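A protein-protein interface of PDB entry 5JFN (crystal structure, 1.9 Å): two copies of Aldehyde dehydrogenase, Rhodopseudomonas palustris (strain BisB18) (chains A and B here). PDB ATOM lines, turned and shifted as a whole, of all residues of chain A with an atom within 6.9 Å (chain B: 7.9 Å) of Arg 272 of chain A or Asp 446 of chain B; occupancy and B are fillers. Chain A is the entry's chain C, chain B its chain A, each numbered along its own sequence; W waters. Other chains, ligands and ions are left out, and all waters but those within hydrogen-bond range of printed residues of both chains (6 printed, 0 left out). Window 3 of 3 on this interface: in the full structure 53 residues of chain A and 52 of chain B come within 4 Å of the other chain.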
ATOM      1  N   PHE A 188     -13.155  10.929 -18.202  1.00  0.00           N
ATOM      2  CA  PHE A 188     -12.451  10.513 -19.410  1.00  0.00           C
ATOM      3  C   PHE A 188     -11.585   9.290 -19.144  1.00  0.00           C
ATOM      4  O   PHE A 188     -11.612   8.316 -19.911  1.00  0.00           O
ATOM      5  CB  PHE A 188     -11.574  11.651 -19.935  1.00  0.00           C
ATOM      6  CG  PHE A 188     -12.219  12.469 -20.999  1.00  0.00           C
ATOM      7  CD1 PHE A 188     -12.175  12.061 -22.318  1.00  0.00           C
ATOM      8  CD2 PHE A 188     -12.855  13.658 -20.687  1.00  0.00           C
ATOM      9  CE1 PHE A 188     -12.767  12.819 -23.309  1.00  0.00           C
ATOM     10  CE2 PHE A 188     -13.445  14.419 -21.671  1.00  0.00           C
ATOM     11  CZ  PHE A 188     -13.401  13.997 -22.982  1.00  0.00           C
ATOM     12  N   GLY A 189     -10.799   9.339 -18.072  1.00  0.00           N
ATOM     13  CA  GLY A 189      -9.837   8.305 -17.755  1.00  0.00           C
ATOM     14  C   GLY A 189      -8.517   8.916 -17.337  1.00  0.00           C
ATOM     15  O   GLY A 189      -8.475   9.735 -16.416  1.00  0.00           O
ATOM     16  N   VAL A 190      -7.433   8.534 -18.006  1.00  0.00           N
ATOM     17  CA  VAL A 190      -6.131   9.143 -17.765  1.00  0.00           C
ATOM     18  C   VAL A 190      -6.026  10.409 -18.602  1.00  0.00           C
ATOM     19  O   VAL A 190      -6.169  10.366 -19.828  1.00  0.00           O
ATOM     20  CB  VAL A 190      -4.990   8.179 -18.109  1.00  0.00           C
ATOM     21  CG1 VAL A 190      -3.647   8.861 -17.887  1.00  0.00           C
ATOM     22  CG2 VAL A 190      -5.109   6.922 -17.286  1.00  0.00           C
ATOM     23  N   ILE A 191      -5.759  11.531 -17.943  1.00  0.00           N
ATOM     24  CA  ILE A 191      -5.509  12.797 -18.610  1.00  0.00           C
ATOM     25  C   ILE A 191      -4.021  13.109 -18.500  1.00  0.00           C
ATOM     26  O   ILE A 191      -3.442  13.014 -17.409  1.00  0.00           O
ATOM     27  CB  ILE A 191      -6.371  13.917 -18.006  1.00  0.00           C
ATOM     28  CG1 ILE A 191      -7.849  13.592 -18.236  1.00  0.00           C
ATOM     29  CG2 ILE A 191      -5.983  15.274 -18.592  1.00  0.00           C
ATOM     30  CD1 ILE A 191      -8.805  14.551 -17.569  1.00  0.00           C
ATOM     31  N   GLY A 192      -3.409  13.447 -19.624  1.00  0.00           N
ATOM     32  CA  GLY A 192      -2.040  13.914 -19.653  1.00  0.00           C
ATOM     33  C   GLY A 192      -2.048  15.426 -19.711  1.00  0.00           C
ATOM     34  O   GLY A 192      -2.624  16.017 -20.626  1.00  0.00           O
ATOM     35  N   ASN A 216     -11.112  11.497 -12.982  1.00  0.00           N
ATOM     36  CA  ASN A 216      -9.942  11.124 -13.760  1.00  0.00           C
ATOM     37  C   ASN A 216      -8.727  10.935 -12.862  1.00  0.00           C
ATOM     38  O   ASN A 216      -8.701  11.360 -11.705  1.00  0.00           O
ATOM     39  CB  ASN A 216      -9.621  12.201 -14.797  1.00  0.00           C
ATOM     40  CG  ASN A 216     -10.802  12.541 -15.670  1.00  0.00           C
ATOM     41  OD1 ASN A 216     -11.160  11.783 -16.573  1.00  0.00           O
ATOM     42  ND2 ASN A 216     -11.419  13.691 -15.409  1.00  0.00           N
ATOM     43  N   HIS A 268       1.106   8.173 -25.831  1.00  0.00           N
ATOM     44  CA  HIS A 268       0.827   6.948 -25.092  1.00  0.00           C
ATOM     45  C   HIS A 268      -0.610   6.494 -25.328  1.00  0.00           C
ATOM     46  O   HIS A 268      -1.543   7.274 -25.113  1.00  0.00           O
ATOM     47  CB  HIS A 268       1.079   7.138 -23.601  1.00  0.00           C
ATOM     48  CG  HIS A 268       1.231   5.847 -22.862  1.00  0.00           C
ATOM     49  ND1 HIS A 268       0.186   4.967 -22.685  1.00  0.00           N
ATOM     50  CD2 HIS A 268       2.311   5.271 -22.283  1.00  0.00           C
ATOM     51  CE1 HIS A 268       0.614   3.907 -22.023  1.00  0.00           C
ATOM     52  NE2 HIS A 268       1.897   4.069 -21.762  1.00  0.00           N
ATOM     53  N   PRO A 269      -0.825   5.240 -25.738  1.00  0.00           N
ATOM     54  CA  PRO A 269      -2.193   4.777 -26.038  1.00  0.00           C
ATOM     55  C   PRO A 269      -3.171   4.903 -24.882  1.00  0.00           C
ATOM     56  O   PRO A 269      -4.379   5.001 -25.118  1.00  0.00           O
ATOM     57  CB  PRO A 269      -1.984   3.303 -26.421  1.00  0.00           C
ATOM     58  CG  PRO A 269      -0.562   3.220 -26.870  1.00  0.00           C
ATOM     59  CD  PRO A 269       0.189   4.212 -26.028  1.00  0.00           C
ATOM     60  N   LYS A 270      -2.699   4.887 -23.641  1.00  0.00           N
ATOM     61  CA  LYS A 270      -3.607   4.897 -22.502  1.00  0.00           C
ATOM     62  C   LYS A 270      -3.961   6.302 -22.023  1.00  0.00           C
ATOM     63  O   LYS A 270      -4.821   6.445 -21.148  1.00  0.00           O
ATOM     64  CB  LYS A 270      -3.009   4.085 -21.349  1.00  0.00           C
ATOM     65  CG  LYS A 270      -2.864   2.607 -21.683  1.00  0.00           C
ATOM     66  CD  LYS A 270      -2.740   1.750 -20.433  1.00  0.00           C
ATOM     67  CE  LYS A 270      -2.722   0.274 -20.807  1.00  0.00           C
ATOM     68  NZ  LYS A 270      -2.879  -0.583 -19.613  1.00  0.00           N
ATOM     69  N   VAL A 271      -3.335   7.335 -22.570  1.00  0.00           N
ATOM     70  CA  VAL A 271      -3.738   8.705 -22.275  1.00  0.00           C
ATOM     71  C   VAL A 271      -4.989   9.011 -23.090  1.00  0.00           C
ATOM     72  O   VAL A 271      -4.970   8.930 -24.321  1.00  0.00           O
ATOM     73  CB  VAL A 271      -2.611   9.697 -22.588  1.00  0.00           C
ATOM     74  CG1 VAL A 271      -3.110  11.140 -22.432  1.00  0.00           C
ATOM     75  CG2 VAL A 271      -1.418   9.441 -21.671  1.00  0.00           C
ATOM     76  N   ARG A 272      -6.086   9.338 -22.403  1.00  0.00           N
ATOM     77  CA  ARG A 272      -7.369   9.536 -23.074  1.00  0.00           C
ATOM     78  C   ARG A 272      -7.596  10.968 -23.525  1.00  0.00           C
ATOM     79  O   ARG A 272      -8.359  11.198 -24.472  1.00  0.00           O
ATOM     80  CB  ARG A 272      -8.523   9.124 -22.157  1.00  0.00           C
ATOM     81  CG  ARG A 272      -8.471   7.665 -21.725  1.00  0.00           C
ATOM     82  CD  ARG A 272      -8.484   6.729 -22.925  1.00  0.00           C
ATOM     83  NE  ARG A 272      -8.600   5.337 -22.497  1.00  0.00           N
ATOM     84  CZ  ARG A 272      -9.713   4.614 -22.582  1.00  0.00           C
ATOM     85  NH1 ARG A 272     -10.815   5.137 -23.106  1.00  0.00           N
ATOM     86  NH2 ARG A 272      -9.716   3.360 -22.153  1.00  0.00           N
ATOM     87  N   MET A 273      -6.970  11.933 -22.861  1.00  0.00           N
ATOM     88  CA  MET A 273      -7.128  13.339 -23.200  1.00  0.00           C
ATOM     89  C   MET A 273      -5.840  14.060 -22.849  1.00  0.00           C
ATOM     90  O   MET A 273      -5.204  13.754 -21.836  1.00  0.00           O
ATOM     91  CB  MET A 273      -8.314  13.975 -22.454  1.00  0.00           C
ATOM     92  CG  MET A 273      -8.240  15.495 -22.352  1.00  0.00           C
ATOM     93  SD  MET A 273      -9.375  16.214 -21.143  1.00  0.00           S
ATOM     94  CE  MET A 273     -10.784  16.567 -22.162  1.00  0.00           C
ATOM     95  N   LEU A 274      -5.455  15.011 -23.689  1.00  0.00           N
ATOM     96  CA  LEU A 274      -4.318  15.871 -23.412  1.00  0.00           C
ATOM     97  C   LEU A 274      -4.817  17.257 -23.039  1.00  0.00           C
ATOM     98  O   LEU A 274      -5.770  17.768 -23.631  1.00  0.00           O
ATOM     99  CB  LEU A 274      -3.383  15.952 -24.619  1.00  0.00           C
ATOM    100  CG  LEU A 274      -2.747  14.599 -24.939  1.00  0.00           C
ATOM    101  CD1 LEU A 274      -2.219  14.566 -26.360  1.00  0.00           C
ATOM    102  CD2 LEU A 274      -1.643  14.296 -23.931  1.00  0.00           C
ATOM    103  N   LYS A 291      -5.672  12.293 -30.391  1.00  0.00           N
ATOM    104  CA  LYS A 291      -6.386  12.261 -29.125  1.00  0.00           C
ATOM    105  C   LYS A 291      -7.173  13.552 -28.946  1.00  0.00           C
ATOM    106  O   LYS A 291      -6.819  14.598 -29.506  1.00  0.00           O
ATOM    107  CB  LYS A 291      -5.412  12.103 -27.941  1.00  0.00           C
ATOM    108  CG  LYS A 291      -4.501  10.890 -28.023  1.00  0.00           C
ATOM    109  CD  LYS A 291      -3.447  10.921 -26.929  1.00  0.00           C
ATOM    110  CE  LYS A 291      -2.661   9.618 -26.893  1.00  0.00           C
ATOM    111  NZ  LYS A 291      -3.524   8.461 -26.550  1.00  0.00           N
ATOM    112  N   LYS A 292      -8.228  13.495 -28.134  1.00  0.00           N
ATOM    113  CA  LYS A 292      -8.838  14.744 -27.702  1.00  0.00           C
ATOM    114  C   LYS A 292      -7.825  15.556 -26.911  1.00  0.00           C
ATOM    115  O   LYS A 292      -7.120  15.028 -26.046  1.00  0.00           O
ATOM    116  CB  LYS A 292     -10.085  14.524 -26.851  1.00  0.00           C
ATOM    117  CG  LYS A 292     -10.816  15.868 -26.654  1.00  0.00           C
ATOM    118  CD  LYS A 292     -11.727  15.898 -25.463  1.00  0.00           C
ATOM    119  CE  LYS A 292     -12.265  17.310 -25.247  1.00  0.00           C
ATOM    120  NZ  LYS A 292     -13.070  17.820 -26.388  1.00  0.00           N
ATOM    121  N   ALA A 293      -7.748  16.845 -27.215  1.00  0.00           N
ATOM    122  CA  ALA A 293      -6.823  17.726 -26.525  1.00  0.00           C
ATOM    123  C   ALA A 293      -7.499  19.057 -26.245  1.00  0.00           C
ATOM    124  O   ALA A 293      -8.216  19.590 -27.097  1.00  0.00           O
ATOM    125  CB  ALA A 293      -5.542  17.953 -27.339  1.00  0.00           C
ATOM    126  N   ARG A 511     -16.634  13.565 -19.867  1.00  0.00           N
ATOM    127  CA  ARG A 511     -17.424  13.190 -21.030  1.00  0.00           C
ATOM    128  C   ARG A 511     -18.890  13.336 -20.683  1.00  0.00           C
ATOM    129  O   ARG A 511     -19.319  12.957 -19.588  1.00  0.00           O
ATOM    130  CB  ARG A 511     -17.166  11.743 -21.455  1.00  0.00           C
ATOM    131  CG  ARG A 511     -15.732  11.316 -21.478  1.00  0.00           C
ATOM    132  CD  ARG A 511     -15.631   9.800 -21.577  1.00  0.00           C
ATOM    133  NE  ARG A 511     -16.239   9.270 -22.793  1.00  0.00           N
ATOM    134  CZ  ARG A 511     -17.283   8.443 -22.820  1.00  0.00           C
ATOM    135  NH1 ARG A 511     -17.864   8.053 -21.691  1.00  0.00           N
ATOM    136  NH2 ARG A 511     -17.751   8.003 -23.982  1.00  0.00           N
ATOM    137  N   ALA B 298     -16.788   4.667 -33.013  1.00  0.00           N
ATOM    138  CA  ALA B 298     -17.456   3.410 -33.273  1.00  0.00           C
ATOM    139  C   ALA B 298     -18.214   2.970 -32.029  1.00  0.00           C
ATOM    140  O   ALA B 298     -17.990   3.463 -30.918  1.00  0.00           O
ATOM    141  CB  ALA B 298     -16.450   2.335 -33.683  1.00  0.00           C
ATOM    142  N   GLY B 299     -19.136   2.042 -32.231  1.00  0.00           N
ATOM    143  CA  GLY B 299     -19.832   1.409 -31.135  1.00  0.00           C
ATOM    144  C   GLY B 299     -19.989  -0.069 -31.413  1.00  0.00           C
ATOM    145  O   GLY B 299     -19.518  -0.584 -32.429  1.00  0.00           O
ATOM    146  N   ASN B 300     -20.642  -0.737 -30.489  1.00  0.00           N
ATOM    147  CA  ASN B 300     -21.044  -2.127 -30.661  1.00  0.00           C
ATOM    148  C   ASN B 300     -22.128  -2.378 -29.629  1.00  0.00           C
ATOM    149  O   ASN B 300     -21.900  -3.121 -28.669  1.00  0.00           O
ATOM    150  CB  ASN B 300     -19.865  -3.080 -30.466  1.00  0.00           C
ATOM    151  CG  ASN B 300     -20.165  -4.485 -30.965  1.00  0.00           C
ATOM    152  OD1 ASN B 300     -20.870  -4.665 -31.961  1.00  0.00           O
ATOM    153  ND2 ASN B 300     -19.645  -5.486 -30.260  1.00  0.00           N
ATOM    154  N   ALA B 440     -21.834  -7.331 -21.273  1.00  0.00           N
ATOM    155  CA  ALA B 440     -22.128  -6.153 -22.086  1.00  0.00           C
ATOM    156  C   ALA B 440     -20.952  -5.187 -22.088  1.00  0.00           C
ATOM    157  O   ALA B 440     -20.548  -4.682 -23.141  1.00  0.00           O
ATOM    158  CB  ALA B 440     -23.397  -5.472 -21.580  1.00  0.00           C
ATOM    159  N   ILE B 441     -20.379  -4.931 -20.911  1.00  0.00           N
ATOM    160  CA  ILE B 441     -19.206  -4.067 -20.825  1.00  0.00           C
ATOM    161  C   ILE B 441     -18.077  -4.626 -21.676  1.00  0.00           C
ATOM    162  O   ILE B 441     -17.405  -3.897 -22.415  1.00  0.00           O
ATOM    163  CB  ILE B 441     -18.778  -3.915 -19.353  1.00  0.00           C
ATOM    164  CG1 ILE B 441     -19.867  -3.198 -18.548  1.00  0.00           C
ATOM    165  CG2 ILE B 441     -17.435  -3.209 -19.248  1.00  0.00           C
ATOM    166  CD1 ILE B 441     -19.695  -3.370 -17.033  1.00  0.00           C
ATOM    167  N   GLU B 442     -17.866  -5.938 -21.601  1.00  0.00           N
ATOM    168  CA  GLU B 442     -16.762  -6.553 -22.325  1.00  0.00           C
ATOM    169  C   GLU B 442     -16.947  -6.432 -23.834  1.00  0.00           C
ATOM    170  O   GLU B 442     -16.048  -5.969 -24.543  1.00  0.00           O
ATOM    171  CB  GLU B 442     -16.632  -8.014 -21.902  1.00  0.00           C
ATOM    172  CG  GLU B 442     -15.552  -8.778 -22.616  1.00  0.00           C
ATOM    173  CD  GLU B 442     -15.354 -10.148 -22.011  1.00  0.00           C
ATOM    174  OE1 GLU B 442     -14.708 -10.235 -20.948  1.00  0.00           O
ATOM    175  OE2 GLU B 442     -15.878 -11.124 -22.576  1.00  0.00           O
ATOM    176  N   VAL B 443     -18.114  -6.837 -24.347  1.00  0.00           N
ATOM    177  CA  VAL B 443     -18.310  -6.830 -25.799  1.00  0.00           C
ATOM    178  C   VAL B 443     -18.533  -5.434 -26.355  1.00  0.00           C
ATOM    179  O   VAL B 443     -18.435  -5.245 -27.572  1.00  0.00           O
ATOM    180  CB  VAL B 443     -19.477  -7.735 -26.235  1.00  0.00           C
ATOM    181  CG1 VAL B 443     -19.302  -9.133 -25.662  1.00  0.00           C
ATOM    182  CG2 VAL B 443     -20.811  -7.135 -25.821  1.00  0.00           C
ATOM    183  N   GLU B 444     -18.811  -4.443 -25.505  1.00  0.00           N
ATOM    184  CA  GLU B 444     -18.879  -3.071 -25.993  1.00  0.00           C
ATOM    185  C   GLU B 444     -17.496  -2.511 -26.318  1.00  0.00           C
ATOM    186  O   GLU B 444     -17.406  -1.454 -26.955  1.00  0.00           O
ATOM    187  CB  GLU B 444     -19.597  -2.176 -24.976  1.00  0.00           C
ATOM    188  CG  GLU B 444     -20.300  -0.952 -25.601  1.00  0.00           C
ATOM    189  CD  GLU B 444     -19.434   0.305 -25.630  1.00  0.00           C
ATOM    190  OE1 GLU B 444     -18.452   0.389 -24.854  1.00  0.00           O
ATOM    191  OE2 GLU B 444     -19.743   1.218 -26.437  1.00  0.00           O
ATOM    192  N   HIS B 445     -16.428  -3.195 -25.896  1.00  0.00           N
ATOM    193  CA  HIS B 445     -15.061  -2.955 -26.363  1.00  0.00           C
ATOM    194  C   HIS B 445     -14.523  -1.592 -25.948  1.00  0.00           C
ATOM    195  O   HIS B 445     -13.659  -1.035 -26.628  1.00  0.00           O
ATOM    196  CB  HIS B 445     -14.952  -3.121 -27.885  1.00  0.00           C
ATOM    197  CG  HIS B 445     -15.220  -4.515 -28.358  1.00  0.00           C
ATOM    198  ND1 HIS B 445     -15.899  -4.789 -29.527  1.00  0.00           N
ATOM    199  CD2 HIS B 445     -14.901  -5.715 -27.818  1.00  0.00           C
ATOM    200  CE1 HIS B 445     -15.989  -6.098 -29.684  1.00  0.00           C
ATOM    201  NE2 HIS B 445     -15.388  -6.683 -28.664  1.00  0.00           N
ATOM    202  N   ASP B 446     -15.016  -1.043 -24.838  1.00  0.00           N
ATOM    203  CA  ASP B 446     -14.587   0.267 -24.345  1.00  0.00           C
ATOM    204  C   ASP B 446     -14.785   1.360 -25.392  1.00  0.00           C
ATOM    205  O   ASP B 446     -14.103   2.390 -25.368  1.00  0.00           O
ATOM    206  CB  ASP B 446     -13.128   0.224 -23.867  1.00  0.00           C
ATOM    207  CG  ASP B 446     -12.700   1.490 -23.129  1.00  0.00           C
ATOM    208  OD1 ASP B 446     -13.526   2.099 -22.420  1.00  0.00           O
ATOM    209  OD2 ASP B 446     -11.524   1.876 -23.271  1.00  0.00           O
ATOM    210  N   ASN B 447     -15.701   1.150 -26.341  1.00  0.00           N
ATOM    211  CA  ASN B 447     -16.134   2.262 -27.173  1.00  0.00           C
ATOM    212  C   ASN B 447     -16.839   3.314 -26.332  1.00  0.00           C
ATOM    213  O   ASN B 447     -16.811   4.506 -26.672  1.00  0.00           O
ATOM    214  CB  ASN B 447     -17.055   1.766 -28.290  1.00  0.00           C
ATOM    215  CG  ASN B 447     -16.310   0.994 -29.361  1.00  0.00           C
ATOM    216  OD1 ASN B 447     -15.309   1.466 -29.888  1.00  0.00           O
ATOM    217  ND2 ASN B 447     -16.789  -0.207 -29.677  1.00  0.00           N
ATOM    218  N   ARG B 448     -17.463   2.889 -25.229  1.00  0.00           N
ATOM    219  CA  ARG B 448     -18.282   3.756 -24.382  1.00  0.00           C
ATOM    220  C   ARG B 448     -19.260   4.567 -25.224  1.00  0.00           C
ATOM    221  O   ARG B 448     -19.479   5.760 -25.001  1.00  0.00           O
ATOM    222  CB  ARG B 448     -17.405   4.662 -23.512  1.00  0.00           C
ATOM    223  CG  ARG B 448     -16.610   3.897 -22.458  1.00  0.00           C
ATOM    224  CD  ARG B 448     -15.924   4.848 -21.482  1.00  0.00           C
ATOM    225  NE  ARG B 448     -14.854   5.619 -22.114  1.00  0.00           N
ATOM    226  CZ  ARG B 448     -14.122   6.531 -21.480  1.00  0.00           C
ATOM    227  NH1 ARG B 448     -14.355   6.792 -20.198  1.00  0.00           N
ATOM    228  NH2 ARG B 448     -13.161   7.181 -22.122  1.00  0.00           N
ATOM    229  N   HIS B 449     -19.856   3.907 -26.213  1.00  0.00           N
ATOM    230  CA  HIS B 449     -20.727   4.606 -27.143  1.00  0.00           C
ATOM    231  C   HIS B 449     -22.186   4.500 -26.710  1.00  0.00           C
ATOM    232  O   HIS B 449     -22.753   5.460 -26.182  1.00  0.00           O
ATOM    233  CB  HIS B 449     -20.538   4.060 -28.566  1.00  0.00           C
ATOM    234  CG  HIS B 449     -21.196   4.899 -29.611  1.00  0.00           C
ATOM    235  ND1 HIS B 449     -22.564   4.994 -29.733  1.00  0.00           N
ATOM    236  CD2 HIS B 449     -20.676   5.707 -30.566  1.00  0.00           C
ATOM    237  CE1 HIS B 449     -22.860   5.816 -30.723  1.00  0.00           C
ATOM    238  NE2 HIS B 449     -21.732   6.261 -31.247  1.00  0.00           N
ATOM    239  N   ILE B 468     -21.189   0.814 -17.366  1.00  0.00           N
ATOM    240  CA  ILE B 468     -20.789   0.718 -18.769  1.00  0.00           C
ATOM    241  C   ILE B 468     -20.360   2.069 -19.345  1.00  0.00           C
ATOM    242  O   ILE B 468     -19.676   2.100 -20.379  1.00  0.00           O
ATOM    243  CB  ILE B 468     -21.901   0.072 -19.615  1.00  0.00           C
ATOM    244  CG1 ILE B 468     -21.313  -0.492 -20.915  1.00  0.00           C
ATOM    245  CG2 ILE B 468     -23.038   1.066 -19.911  1.00  0.00           C
ATOM    246  CD1 ILE B 468     -22.202  -1.529 -21.592  1.00  0.00           C
ATOM    247  N   GLN B 469     -20.736   3.177 -18.704  1.00  0.00           N
ATOM    248  CA  GLN B 469     -20.160   4.499 -18.979  1.00  0.00           C
ATOM    249  C   GLN B 469     -20.287   4.900 -20.451  1.00  0.00           C
ATOM    250  O   GLN B 469     -19.384   5.507 -21.027  1.00  0.00           O
ATOM    251  CB  GLN B 469     -18.698   4.553 -18.527  1.00  0.00           C
ATOM    252  CG  GLN B 469     -18.529   4.554 -17.005  1.00  0.00           C
ATOM    253  CD  GLN B 469     -18.785   5.923 -16.403  1.00  0.00           C
ATOM    254  OE1 GLN B 469     -18.136   6.902 -16.775  1.00  0.00           O
ATOM    255  NE2 GLN B 469     -19.747   6.007 -15.482  1.00  0.00           N
ATOM    256  N   THR B 470     -21.419   4.580 -21.063  1.00  0.00           N
ATOM    257  CA  THR B 470     -21.609   4.893 -22.472  1.00  0.00           C
ATOM    258  C   THR B 470     -22.165   6.301 -22.657  1.00  0.00           C
ATOM    259  O   THR B 470     -22.884   6.832 -21.805  1.00  0.00           O
ATOM    260  CB  THR B 470     -22.546   3.892 -23.141  1.00  0.00           C
ATOM    261  OG1 THR B 470     -23.750   3.780 -22.373  1.00  0.00           O
ATOM    262  CG2 THR B 470     -21.875   2.527 -23.275  1.00  0.00           C
ATOM    263  N   PRO B 498     -14.260   9.856 -29.094  1.00  0.00           N
ATOM    264  CA  PRO B 498     -13.131  10.144 -28.203  1.00  0.00           C
ATOM    265  C   PRO B 498     -13.158  11.538 -27.606  1.00  0.00           C
ATOM    266  O   PRO B 498     -12.470  11.759 -26.604  1.00  0.00           O
ATOM    267  CB  PRO B 498     -11.908   9.956 -29.114  1.00  0.00           C
ATOM    268  CG  PRO B 498     -12.430  10.190 -30.494  1.00  0.00           C
ATOM    269  CD  PRO B 498     -13.832   9.648 -30.487  1.00  0.00           C
ATOM    270  N   THR B 499     -13.923  12.480 -28.164  1.00  0.00           N
ATOM    271  CA  THR B 499     -13.795  13.877 -27.768  1.00  0.00           C
ATOM    272  C   THR B 499     -14.812  14.309 -26.714  1.00  0.00           C
ATOM    273  O   THR B 499     -14.728  15.438 -26.226  1.00  0.00           O
ATOM    274  CB  THR B 499     -13.868  14.793 -29.003  1.00  0.00           C
ATOM    275  OG1 THR B 499     -15.047  14.506 -29.763  1.00  0.00           O
ATOM    276  CG2 THR B 499     -12.641  14.580 -29.885  1.00  0.00           C
HETATM  277  O   HOH W   1     -11.869   7.730 -24.973  1.00  0.00           O
HETATM  278  O   HOH W   2     -17.237   8.453 -19.004  1.00  0.00           O
HETATM  279  O   HOH W   3     -16.551   7.217 -26.518  1.00  0.00           O
HETATM  280  O   HOH W   4     -15.730  17.471 -24.602  1.00  0.00           O
HETATM  281  O   HOH W   5     -10.871  10.217 -25.114  1.00  0.00           O
HETATM  282  O   HOH W   6     -13.567   5.017 -24.649  1.00  0.00           O
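Water W5 lies within hydrogen-bond range of the backbone carbonyl oxygen of Pro 498 of chain B (2.7 Å) and the backbone carbonyl oxygen of Arg 272 of chain A (2.8 Å). Water W3 bridges the backbone carbonyl oxygen (O) of Asn 447 of chain B (2.7 Å) and the guanidinium group (NH2) of Arg 511 of chain A (2.9 Å). Water W6 lies within hydrogen-bond range of O of Asp 446 of chain B (2.8 Å), NE of Arg 448 of chain B (2.9 Å) and NH1 of Arg 272 of chain A (3.2 Å). Water W2 lies within hydrogen-bond range of the guanidinium group (NH1) of Arg 511 of chain A (2.8 Å) and the side-chain amide oxygen (OE1) of Gln 469 of chain B (2.9 Å). Water W4 lies within hydrogen-bond range of O of Thr 499 of chain B and NZ of Lys 292 of chain A. Water W1 lies within hydrogen-bond range of NH2 of Arg 448 of chain B (3.2 Å) and NH1 of Arg 272 of chain A (3.4 Å).
Among the printed residues, pairs that only touch across the chains: Phe 188 of chain A with Pro 498 of chain B, Lys 292 of chain A with Pro 498 of chain B and Phe 188 of chain A with Thr 499 of chain B.
No position is printed for both chains.
Of the printed residues of chain B, Phe 188 of chain A touches Arg 448 (2.9 Å), Pro 498 (3.5 Å) and Thr 499 (3.8 Å). Arg 272 of chain A touches just these residues of chain B: Asp 446 (2.6 Å) and Arg 448 (3.3 Å). Of the printed residues of chain B, Lys 292 of chain A touches Pro 498 (3.7 Å) and Thr 499 (2.9 Å). Of the printed residues of chain B, Arg 511 of chain A touches Arg 448 (3.0 Å) and Gln 469 (3.0 Å). Of chain A, only Arg 272 comes within 4 Å of Asp 446 of chain B. Of the printed residues of chain A, Arg 448 of chain B touches Phe 188, Arg 272 and Arg 511. Of the printed residues of chain A, Pro 498 of chain B touches Phe 188 (3.5 Å) and Lys 292 (3.7 Å). The nearest residue of chain B that does not touch Arg 272 of chain A is Pro 498 of chain B (4.7 Å). The nearest printed residue of chain B that does not touch Phe 188 of chain A is Gln 469 of chain B (6.6 Å).
OD1 of Asn 216 of chain A is in hydrogen-bond range of N of Phe 188 of chain A, at 2.7 Å. OE1 of Glu 444 of chain B lies within hydrogen-bond range of N of Arg 448 of chain B (2.7 Å). The backbone carbonyl oxygen (O) of Lys 292 of chain A lies within hydrogen-bond range of the backbone NH (N) of Leu 274 of chain A. O of Val 190 of chain A sits at hydrogen-bond distance from N of Arg 272 of chain A (2.8 Å). NE of Arg 448 of chain B is in salt-bridge range of OD1 of Asp 446 of chain B (3.8 Å).
The backbone carbonyl oxygen (O) of Phe 188 of chain A sits at hydrogen-bond distance from the guanidinium group (NH2) of Arg 448 of chain B, at 2.9 Å. NH1 of Arg 272 of chain A lies close to NH2 of Arg 448 of chain B (3.3 Å). NZ of Lys 292 of chain A lies within hydrogen-bond range of O of Thr 499 of chain B (2.9 Å). The backbone carbonyl oxygen of Arg 448 of chain B lies within hydrogen-bond range of the guanidinium group of Arg 511 of chain A (3.0 Å). O of Gln 469 of chain B lies within hydrogen-bond range of NH1 of Arg 511 of chain A (3.0 Å). OD2 of Asp 446 of chain B lies within salt-bridge range of NH2 of Arg 272 of chain A (2.6 Å).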
